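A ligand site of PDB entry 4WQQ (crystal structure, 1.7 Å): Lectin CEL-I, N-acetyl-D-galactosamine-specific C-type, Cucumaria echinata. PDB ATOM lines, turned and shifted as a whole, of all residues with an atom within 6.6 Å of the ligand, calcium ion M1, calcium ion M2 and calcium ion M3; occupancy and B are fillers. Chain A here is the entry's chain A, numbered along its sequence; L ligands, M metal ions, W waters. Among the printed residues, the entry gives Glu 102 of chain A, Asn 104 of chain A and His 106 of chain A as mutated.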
ATOM      1  N   ASP A  78      -4.264 -19.165   3.906  1.00  0.00           N
ATOM      2  CA  ASP A  78      -4.734 -18.616   5.183  1.00  0.00           C
ATOM      3  C   ASP A  78      -4.593 -19.592   6.366  1.00  0.00           C
ATOM      4  O   ASP A  78      -5.432 -19.641   7.265  1.00  0.00           O
ATOM      5  CB  ASP A  78      -6.178 -18.123   5.046  1.00  0.00           C
ATOM      6  CG  ASP A  78      -7.225 -19.264   4.984  1.00  0.00           C
ATOM      7  OD1 ASP A  78      -6.954 -20.359   4.508  1.00  0.00           O
ATOM      8  OD2 ASP A  78      -8.365 -19.055   5.385  1.00  0.00           O
ATOM      9  N   LYS A  79      -3.530 -20.385   6.313  1.00  0.00           N
ATOM     10  CA  LYS A  79      -3.124 -21.270   7.372  1.00  0.00           C
ATOM     11  C   LYS A  79      -2.994 -20.553   8.719  1.00  0.00           C
ATOM     12  O   LYS A  79      -3.444 -21.064   9.711  1.00  0.00           O
ATOM     13  CB  LYS A  79      -1.774 -21.938   7.053  1.00  0.00           C
ATOM     14  CG  LYS A  79      -1.312 -22.868   8.129  1.00  0.00           C
ATOM     15  CD  LYS A  79       0.003 -23.597   7.842  1.00  0.00           C
ATOM     16  CE  LYS A  79       0.472 -24.195   9.182  1.00  0.00           C
ATOM     17  NZ  LYS A  79       1.368 -25.336   8.944  1.00  0.00           N
ATOM     18  N   ASN A  81      -3.966 -17.343   9.712  1.00  0.00           N
ATOM     19  CA  ASN A  81      -5.082 -16.529  10.059  1.00  0.00           C
ATOM     20  C   ASN A  81      -6.213 -16.843   9.131  1.00  0.00           C
ATOM     21  O   ASN A  81      -6.300 -16.291   8.038  1.00  0.00           O
ATOM     22  CB  ASN A  81      -4.743 -15.049  10.037  1.00  0.00           C
ATOM     23  CG  ASN A  81      -3.966 -14.630  11.264  1.00  0.00           C
ATOM     24  OD1 ASN A  81      -4.561 -14.316  12.332  1.00  0.00           O
ATOM     25  ND2 ASN A  81      -2.683 -14.696  11.168  1.00  0.00           N
ATOM     26  N   GLU A  82      -7.028 -17.820   9.537  1.00  0.00           N
ATOM     27  CA  GLU A  82      -8.181 -18.220   8.753  1.00  0.00           C
ATOM     28  C   GLU A  82      -9.009 -17.057   8.273  1.00  0.00           C
ATOM     29  O   GLU A  82      -9.471 -16.224   9.078  1.00  0.00           O
ATOM     30  CB  GLU A  82      -9.048 -19.218   9.532  1.00  0.00           C
ATOM     31  CG  GLU A  82     -10.352 -19.702   8.875  1.00  0.00           C
ATOM     32  CD  GLU A  82     -10.117 -20.438   7.571  1.00  0.00           C
ATOM     33  OE1 GLU A  82     -10.873 -20.145   6.607  1.00  0.00           O
ATOM     34  OE2 GLU A  82      -9.155 -21.229   7.530  1.00  0.00           O
ATOM     35  N   GLY A  83      -9.279 -17.025   6.969  1.00  0.00           N
ATOM     36  CA  GLY A  83     -10.080 -15.953   6.370  1.00  0.00           C
ATOM     37  C   GLY A  83      -9.248 -14.760   5.975  1.00  0.00           C
ATOM     38  O   GLY A  83      -9.739 -13.919   5.200  1.00  0.00           O
ATOM     39  N   PHE A  85      -6.149 -14.174   3.936  1.00  0.00           N
ATOM     40  CA  PHE A  85      -5.149 -14.754   3.041  1.00  0.00           C
ATOM     41  C   PHE A  85      -3.942 -13.860   2.941  1.00  0.00           C
ATOM     42  O   PHE A  85      -4.086 -12.646   2.945  1.00  0.00           O
ATOM     43  CB  PHE A  85      -5.766 -15.044   1.665  1.00  0.00           C
ATOM     44  CG  PHE A  85      -6.624 -16.317   1.661  1.00  0.00           C
ATOM     45  CD1 PHE A  85      -7.930 -16.288   2.066  1.00  0.00           C
ATOM     46  CD2 PHE A  85      -6.086 -17.562   1.320  1.00  0.00           C
ATOM     47  CE1 PHE A  85      -8.699 -17.450   2.102  1.00  0.00           C
ATOM     48  CE2 PHE A  85      -6.828 -18.708   1.345  1.00  0.00           C
ATOM     49  CZ  PHE A  85      -8.154 -18.657   1.781  1.00  0.00           C
ATOM     50  N   GLY A 101     -18.669 -17.185  -4.778  1.00  0.00           N
ATOM     51  CA  GLY A 101     -18.735 -17.948  -3.527  1.00  0.00           C
ATOM     52  C   GLY A 101     -17.460 -18.403  -2.852  1.00  0.00           C
ATOM     53  O   GLY A 101     -17.508 -19.045  -1.783  1.00  0.00           O
ATOM     54  N   GLU A 102     -16.311 -18.002  -3.427  1.00  0.00           N
ATOM     55  CA  GLU A 102     -15.023 -18.296  -2.792  1.00  0.00           C
ATOM     56  C   GLU A 102     -14.495 -17.011  -2.101  1.00  0.00           C
ATOM     57  O   GLU A 102     -14.860 -15.889  -2.560  1.00  0.00           O
ATOM     58  CB  GLU A 102     -14.060 -18.751  -3.884  1.00  0.00           C
ATOM     59  CG  GLU A 102     -14.625 -19.890  -4.705  1.00  0.00           C
ATOM     60  CD  GLU A 102     -14.875 -21.215  -3.949  1.00  0.00           C
ATOM     61  OE1 GLU A 102     -14.363 -21.366  -2.828  1.00  0.00           O
ATOM     62  OE2 GLU A 102     -15.579 -22.141  -4.492  1.00  0.00           O
ATOM     63  N   PRO A 103     -13.622 -17.148  -1.097  1.00  0.00           N
ATOM     64  CA  PRO A 103     -13.140 -18.460  -0.541  1.00  0.00           C
ATOM     65  C   PRO A 103     -14.210 -19.020   0.384  1.00  0.00           C
ATOM     66  O   PRO A 103     -14.848 -18.261   1.079  1.00  0.00           O
ATOM     67  CB  PRO A 103     -11.909 -18.063   0.280  1.00  0.00           C
ATOM     68  CG  PRO A 103     -12.122 -16.656   0.647  1.00  0.00           C
ATOM     69  CD  PRO A 103     -12.938 -16.025  -0.454  1.00  0.00           C
ATOM     70  N   ASN A 104     -14.507 -20.287   0.324  1.00  0.00           N
ATOM     71  CA  ASN A 104     -15.555 -20.821   1.160  1.00  0.00           C
ATOM     72  C   ASN A 104     -15.081 -21.741   2.253  1.00  0.00           C
ATOM     73  O   ASN A 104     -15.900 -22.281   2.959  1.00  0.00           O
ATOM     74  CB  ASN A 104     -16.588 -21.507   0.294  1.00  0.00           C
ATOM     75  CG  ASN A 104     -16.083 -22.747  -0.412  1.00  0.00           C
ATOM     76  OD1 ASN A 104     -14.905 -23.046  -0.424  1.00  0.00           O
ATOM     77  ND2 ASN A 104     -16.975 -23.454  -1.041  1.00  0.00           N
ATOM     78  N   ASN A 105     -13.771 -21.969   2.390  1.00  0.00           N
ATOM     79  CA  ASN A 105     -13.222 -22.813   3.467  1.00  0.00           C
ATOM     80  C   ASN A 105     -14.008 -24.121   3.574  1.00  0.00           C
ATOM     81  O   ASN A 105     -14.388 -24.564   4.664  1.00  0.00           O
ATOM     82  CB  ASN A 105     -13.193 -22.038   4.798  1.00  0.00           C
ATOM     83  CG  ASN A 105     -12.253 -22.643   5.785  1.00  0.00           C
ATOM     84  OD1 ASN A 105     -11.088 -23.047   5.485  1.00  0.00           O
ATOM     85  ND2 ASN A 105     -12.717 -22.731   7.018  1.00  0.00           N
ATOM     86  N   HIS A 106     -14.218 -24.757   2.423  1.00  0.00           N
ATOM     87  CA  HIS A 106     -15.194 -25.846   2.364  1.00  0.00           C
ATOM     88  C   HIS A 106     -14.833 -26.933   3.357  1.00  0.00           C
ATOM     89  O   HIS A 106     -13.658 -27.251   3.606  1.00  0.00           O
ATOM     90  CB  HIS A 106     -15.249 -26.431   0.960  1.00  0.00           C
ATOM     91  CG  HIS A 106     -16.257 -27.512   0.809  1.00  0.00           C
ATOM     92  ND1 HIS A 106     -17.589 -27.235   0.664  1.00  0.00           N
ATOM     93  CD2 HIS A 106     -16.127 -28.852   0.736  1.00  0.00           C
ATOM     94  CE1 HIS A 106     -18.260 -28.363   0.500  1.00  0.00           C
ATOM     95  NE2 HIS A 106     -17.394 -29.360   0.576  1.00  0.00           N
ATOM     96  N   ASN A 108     -14.582 -26.703   6.380  1.00  0.00           N
ATOM     97  CA  ASN A 108     -13.685 -26.133   7.332  1.00  0.00           C
ATOM     98  C   ASN A 108     -12.217 -26.444   7.147  1.00  0.00           C
ATOM     99  O   ASN A 108     -11.495 -26.428   8.127  1.00  0.00           O
ATOM    100  CB  ASN A 108     -14.032 -26.541   8.786  1.00  0.00           C
ATOM    101  CG  ASN A 108     -15.324 -25.964   9.229  1.00  0.00           C
ATOM    102  OD1 ASN A 108     -15.364 -24.955   9.928  1.00  0.00           O
ATOM    103  ND2 ASN A 108     -16.399 -26.581   8.837  1.00  0.00           N
ATOM    104  N   ALA A 109     -11.766 -26.695   5.914  1.00  0.00           N
ATOM    105  CA  ALA A 109     -10.463 -27.254   5.637  1.00  0.00           C
ATOM    106  C   ALA A 109      -9.918 -26.870   4.286  1.00  0.00           C
ATOM    107  O   ALA A 109      -9.539 -27.732   3.518  1.00  0.00           O
ATOM    108  CB  ALA A 109     -10.535 -28.770   5.711  1.00  0.00           C
ATOM    109  N   GLU A 110      -9.976 -25.593   3.951  1.00  0.00           N
ATOM    110  CA  GLU A 110      -9.410 -25.139   2.704  1.00  0.00           C
ATOM    111  C   GLU A 110      -8.628 -23.887   2.982  1.00  0.00           C
ATOM    112  O   GLU A 110      -9.195 -22.778   3.174  1.00  0.00           O
ATOM    113  CB  GLU A 110     -10.479 -24.920   1.621  1.00  0.00           C
ATOM    114  CG  GLU A 110     -11.193 -26.188   1.171  1.00  0.00           C
ATOM    115  CD  GLU A 110     -12.017 -25.966  -0.085  1.00  0.00           C
ATOM    116  OE1 GLU A 110     -12.680 -24.886  -0.157  1.00  0.00           O
ATOM    117  OE2 GLU A 110     -12.049 -26.866  -0.977  1.00  0.00           O
ATOM    118  N   ASP A 111      -7.298 -24.045   2.937  1.00  0.00           N
ATOM    119  CA  ASP A 111      -6.420 -22.955   3.237  1.00  0.00           C
ATOM    120  C   ASP A 111      -5.496 -22.487   2.080  1.00  0.00           C
ATOM    121  O   ASP A 111      -4.619 -21.690   2.286  1.00  0.00           O
ATOM    122  CB  ASP A 111      -5.607 -23.252   4.502  1.00  0.00           C
ATOM    123  CG  ASP A 111      -6.468 -23.293   5.817  1.00  0.00           C
ATOM    124  OD1 ASP A 111      -7.713 -22.984   5.836  1.00  0.00           O
ATOM    125  OD2 ASP A 111      -5.853 -23.631   6.870  1.00  0.00           O
ATOM    126  N   TYR A 112      -5.672 -23.008   0.882  1.00  0.00           N
ATOM    127  CA  TYR A 112      -4.653 -22.906  -0.183  1.00  0.00           C
ATOM    128  C   TYR A 112      -5.274 -22.412  -1.464  1.00  0.00           C
ATOM    129  O   TYR A 112      -6.214 -23.019  -1.994  1.00  0.00           O
ATOM    130  CB  TYR A 112      -3.858 -24.247  -0.353  1.00  0.00           C
ATOM    131  CG  TYR A 112      -3.304 -24.642   0.948  1.00  0.00           C
ATOM    132  CD1 TYR A 112      -2.205 -23.948   1.481  1.00  0.00           C
ATOM    133  CD2 TYR A 112      -3.985 -25.555   1.774  1.00  0.00           C
ATOM    134  CE1 TYR A 112      -1.741 -24.208   2.742  1.00  0.00           C
ATOM    135  CE2 TYR A 112      -3.515 -25.817   3.056  1.00  0.00           C
ATOM    136  CZ  TYR A 112      -2.392 -25.160   3.513  1.00  0.00           C
ATOM    137  OH  TYR A 112      -1.948 -25.441   4.821  1.00  0.00           O
ATOM    138  N   GLN A 114      -5.722 -21.167  -5.511  1.00  0.00           N
ATOM    139  CA  GLN A 114      -5.432 -21.700  -6.812  1.00  0.00           C
ATOM    140  C   GLN A 114      -6.315 -20.975  -7.865  1.00  0.00           C
ATOM    141  O   GLN A 114      -7.428 -20.545  -7.546  1.00  0.00           O
ATOM    142  CB  GLN A 114      -5.687 -23.237  -6.867  1.00  0.00           C
ATOM    143  CG  GLN A 114      -7.125 -23.640  -6.530  1.00  0.00           C
ATOM    144  CD  GLN A 114      -7.431 -25.121  -6.457  1.00  0.00           C
ATOM    145  OE1 GLN A 114      -8.597 -25.427  -6.412  1.00  0.00           O
ATOM    146  NE2 GLN A 114      -6.454 -26.013  -6.348  1.00  0.00           N
ATOM    147  N   ARG A 116      -8.823 -21.454 -10.965  1.00  0.00           N
ATOM    148  CA  ARG A 116      -9.607 -22.312 -11.856  1.00  0.00           C
ATOM    149  C   ARG A 116      -9.166 -22.144 -13.314  1.00  0.00           C
ATOM    150  O   ARG A 116      -8.563 -21.146 -13.672  1.00  0.00           O
ATOM    151  CB  ARG A 116     -11.102 -21.893 -11.742  1.00  0.00           C
ATOM    152  CG  ARG A 116     -11.523 -21.992 -10.316  1.00  0.00           C
ATOM    153  CD  ARG A 116     -12.960 -22.264 -10.102  1.00  0.00           C
ATOM    154  NE  ARG A 116     -13.038 -23.561  -9.424  1.00  0.00           N
ATOM    155  CZ  ARG A 116     -13.715 -23.812  -8.292  1.00  0.00           C
ATOM    156  NH1 ARG A 116     -14.460 -22.862  -7.621  1.00  0.00           N
ATOM    157  NH2 ARG A 116     -13.650 -25.046  -7.815  1.00  0.00           N
ATOM    158  N   ASN A 124      -9.984 -20.071  -6.301  1.00  0.00           N
ATOM    159  CA  ASN A 124     -10.626 -20.916  -5.335  1.00  0.00           C
ATOM    160  C   ASN A 124      -9.621 -21.245  -4.205  1.00  0.00           C
ATOM    161  O   ASN A 124      -8.405 -21.301  -4.445  1.00  0.00           O
ATOM    162  CB  ASN A 124     -11.012 -22.189  -6.020  1.00  0.00           C
ATOM    163  CG  ASN A 124     -11.645 -23.172  -5.088  1.00  0.00           C
ATOM    164  OD1 ASN A 124     -12.496 -22.844  -4.262  1.00  0.00           O
ATOM    165  ND2 ASN A 124     -11.185 -24.414  -5.181  1.00  0.00           N
ATOM    166  N   ASP A 125     -10.133 -21.429  -2.995  1.00  0.00           N
ATOM    167  CA  ASP A 125      -9.411 -22.051  -1.916  1.00  0.00           C
ATOM    168  C   ASP A 125      -9.642 -23.568  -1.939  1.00  0.00           C
ATOM    169  O   ASP A 125     -10.774 -24.057  -2.157  1.00  0.00           O
ATOM    170  CB  ASP A 125      -9.713 -21.416  -0.550  1.00  0.00           C
ATOM    171  CG  ASP A 125     -11.208 -21.510  -0.147  1.00  0.00           C
ATOM    172  OD1 ASP A 125     -12.122 -21.718  -1.003  1.00  0.00           O
ATOM    173  OD2 ASP A 125     -11.462 -21.310   1.027  1.00  0.00           O
ATOM    174  N   ASN A 126      -8.578 -24.297  -1.654  1.00  0.00           N
ATOM    175  CA  ASN A 126      -8.693 -25.739  -1.649  1.00  0.00           C
ATOM    176  C   ASN A 126      -7.848 -26.303  -0.479  1.00  0.00           C
ATOM    177  O   ASN A 126      -7.175 -25.566   0.270  1.00  0.00           O
ATOM    178  CB  ASN A 126      -8.316 -26.298  -3.030  1.00  0.00           C
ATOM    179  CG  ASN A 126      -9.122 -27.548  -3.422  1.00  0.00           C
ATOM    180  OD1 ASN A 126      -9.442 -28.396  -2.577  1.00  0.00           O
ATOM    181  ND2 ASN A 126      -9.444 -27.687  -4.732  1.00  0.00           N
ATOM    182  N   SER A 127      -7.884 -27.609  -0.330  1.00  0.00           N
ATOM    183  CA  SER A 127      -7.338 -28.232   0.843  1.00  0.00           C
ATOM    184  C   SER A 127      -5.872 -28.643   0.715  1.00  0.00           C
ATOM    185  O   SER A 127      -5.319 -28.637  -0.342  1.00  0.00           O
ATOM    186  CB  SER A 127      -8.157 -29.479   1.130  1.00  0.00           C
ATOM    187  OG  SER A 127      -7.769 -30.488   0.190  1.00  0.00           O
ATOM    188  N   ALA A 130      -5.617 -31.641  -1.767  1.00  0.00           N
ATOM    189  CA  ALA A 130      -5.880 -31.391  -3.160  1.00  0.00           C
ATOM    190  C   ALA A 130      -4.581 -31.293  -3.954  1.00  0.00           C
ATOM    191  O   ALA A 130      -3.489 -31.075  -3.399  1.00  0.00           O
ATOM    192  CB  ALA A 130      -6.667 -30.101  -3.269  1.00  0.00           C
HETATM  193  C1  LIG L   1     -16.197 -27.302  -5.215  1.00  0.00           C
HETATM  194  C2  LIG L   1     -16.330 -25.956  -4.555  1.00  0.00           C
HETATM  195  C3  LIG L   1     -14.980 -25.352  -4.185  1.00  0.00           C
HETATM  196  C4  LIG L   1     -14.135 -26.408  -3.504  1.00  0.00           C
HETATM  197  C5  LIG L   1     -13.922 -27.557  -4.526  1.00  0.00           C
HETATM  198  C6  LIG L   1     -13.024 -28.690  -4.112  1.00  0.00           C
HETATM  199  O1  LIG L   1     -15.767 -26.975  -6.514  1.00  0.00           O
HETATM  200  O2  LIG L   1     -17.024 -26.248  -3.365  1.00  0.00           O
HETATM  201  O3  LIG L   1     -15.239 -24.287  -3.270  1.00  0.00           O
HETATM  202  O4  LIG L   1     -12.926 -25.777  -3.127  1.00  0.00           O
HETATM  203  O5  LIG L   1     -15.244 -28.196  -4.621  1.00  0.00           O
HETATM  204  O6  LIG L   1     -13.605 -28.993  -2.864  1.00  0.00           O
HETATM  205 CA    CA M   1      -9.238 -21.321   5.019  1.00  0.00          CA
HETATM  206 CA    CA M   2     -13.176 -23.464  -2.062  1.00  0.00          CA
HETATM  207 CA    CA M   3      -7.850 -23.147   8.240  1.00  0.00          CA
HETATM  208  O   HOH W   1      -6.554 -21.449   9.048  1.00  0.00           O
HETATM  209  O   HOH W   2     -10.555 -30.785  -2.925  1.00  0.00           O
HETATM  210  O   HOH W   3     -10.606 -20.326   3.391  1.00  0.00           O
HETATM  211  O   HOH W   4     -10.004 -24.172   7.622  1.00  0.00           O
HETATM  212  O   HOH W   5     -11.764 -29.436  -0.355  1.00  0.00           O
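Two residues have an atom within 4 Å of calcium ion M3: Glu 82 and Asp 111.
The nearest printed residue that does not touch calcium ion M3 is Asn 105 (4.3 Å).
The nearest printed residue that does not touch calcium ion M1 is Phe 85 (4.3 Å).
Calcium ion M1 is bound by water W3 (2.3 Å), O of Glu 110 (2.4 Å), OD1 of Asp 111 (2.4 Å), OD2 of Asp 78 (2.5 Å), OE2 of Glu 82 (2.5 Å), OD1 of Asp 78 (2.5 Å), OE1 of Glu 82 (2.6 Å) and OD1 of Asn 105 (2.6 Å).
The guanidinium group (NH2) of Arg 116 is in hydrogen-bond range of an oxygen (O1) of the ligand, at 3.1 Å.
Calcium ion M3 is bound by water W1, the side-chain carboxylate (OD1) of Asp 111, the side-chain carboxylate (OE2) of Glu 82, water W4 and the side-chain carboxylate (OD2) of Asp 111.
Calcium ion M3 has five donor atoms within binding distance.
Merely in contact with the ligand: Asn 126.
Of the 24 residues printed, 7 come within 4 Å of the ligand.
The nearest printed residue that does not touch the ligand is His 106 (4.2 Å).
Calcium ion M2 is bound by OD1 of Asp 125, OD1 of Asn 124, OD1 of Asn 104, OE1 of Glu 110, O of Asp 125, O3 of the ligand, OE1 of Glu 102 and O4 of the ligand.
Water W4 bridges O of Asn 108 (2.8 Å) and ND2 of Asn 105 (3.1 Å).
Water W5 lies within hydrogen-bond range of the side-chain carboxylate (OE2) of Glu 110 (2.7 Å), an oxygen (O6) of the ligand (3.1 Å) and the side-chain amide oxygen (OD1) of Asn 126 (3.4 Å).
The backbone carbonyl oxygen (O) of Asn 126 lies within hydrogen-bond range of the backbone NH (N) of Asp 111 (3.1 Å).
The backbone NH of Asn 105 lies within hydrogen-bond range of the side-chain carboxylate of Asp 125.
O of Tyr 112 sits at hydrogen-bond distance from N of Asn 126.
N of Asn 124 lies within hydrogen-bond range of O of Gln 114 (2.9 Å).
The side-chain carboxylate (OD2) of Asp 78 sits close to the backbone NH (N) of Gly 83 (2.7 Å).
OE1 of Glu 110 sits close to N of His 106 (3.0 Å).
OD1 of Asn 104 sits close to N of His 106 (3.4 Å).
OE2 of Glu 110 lies close to OD1 of Asn 126 (3.4 Å).
Five residues have an atom within 4 Å of calcium ion M2: Glu 102, Asn 104, Glu 110, Asn 124 and Asp 125.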
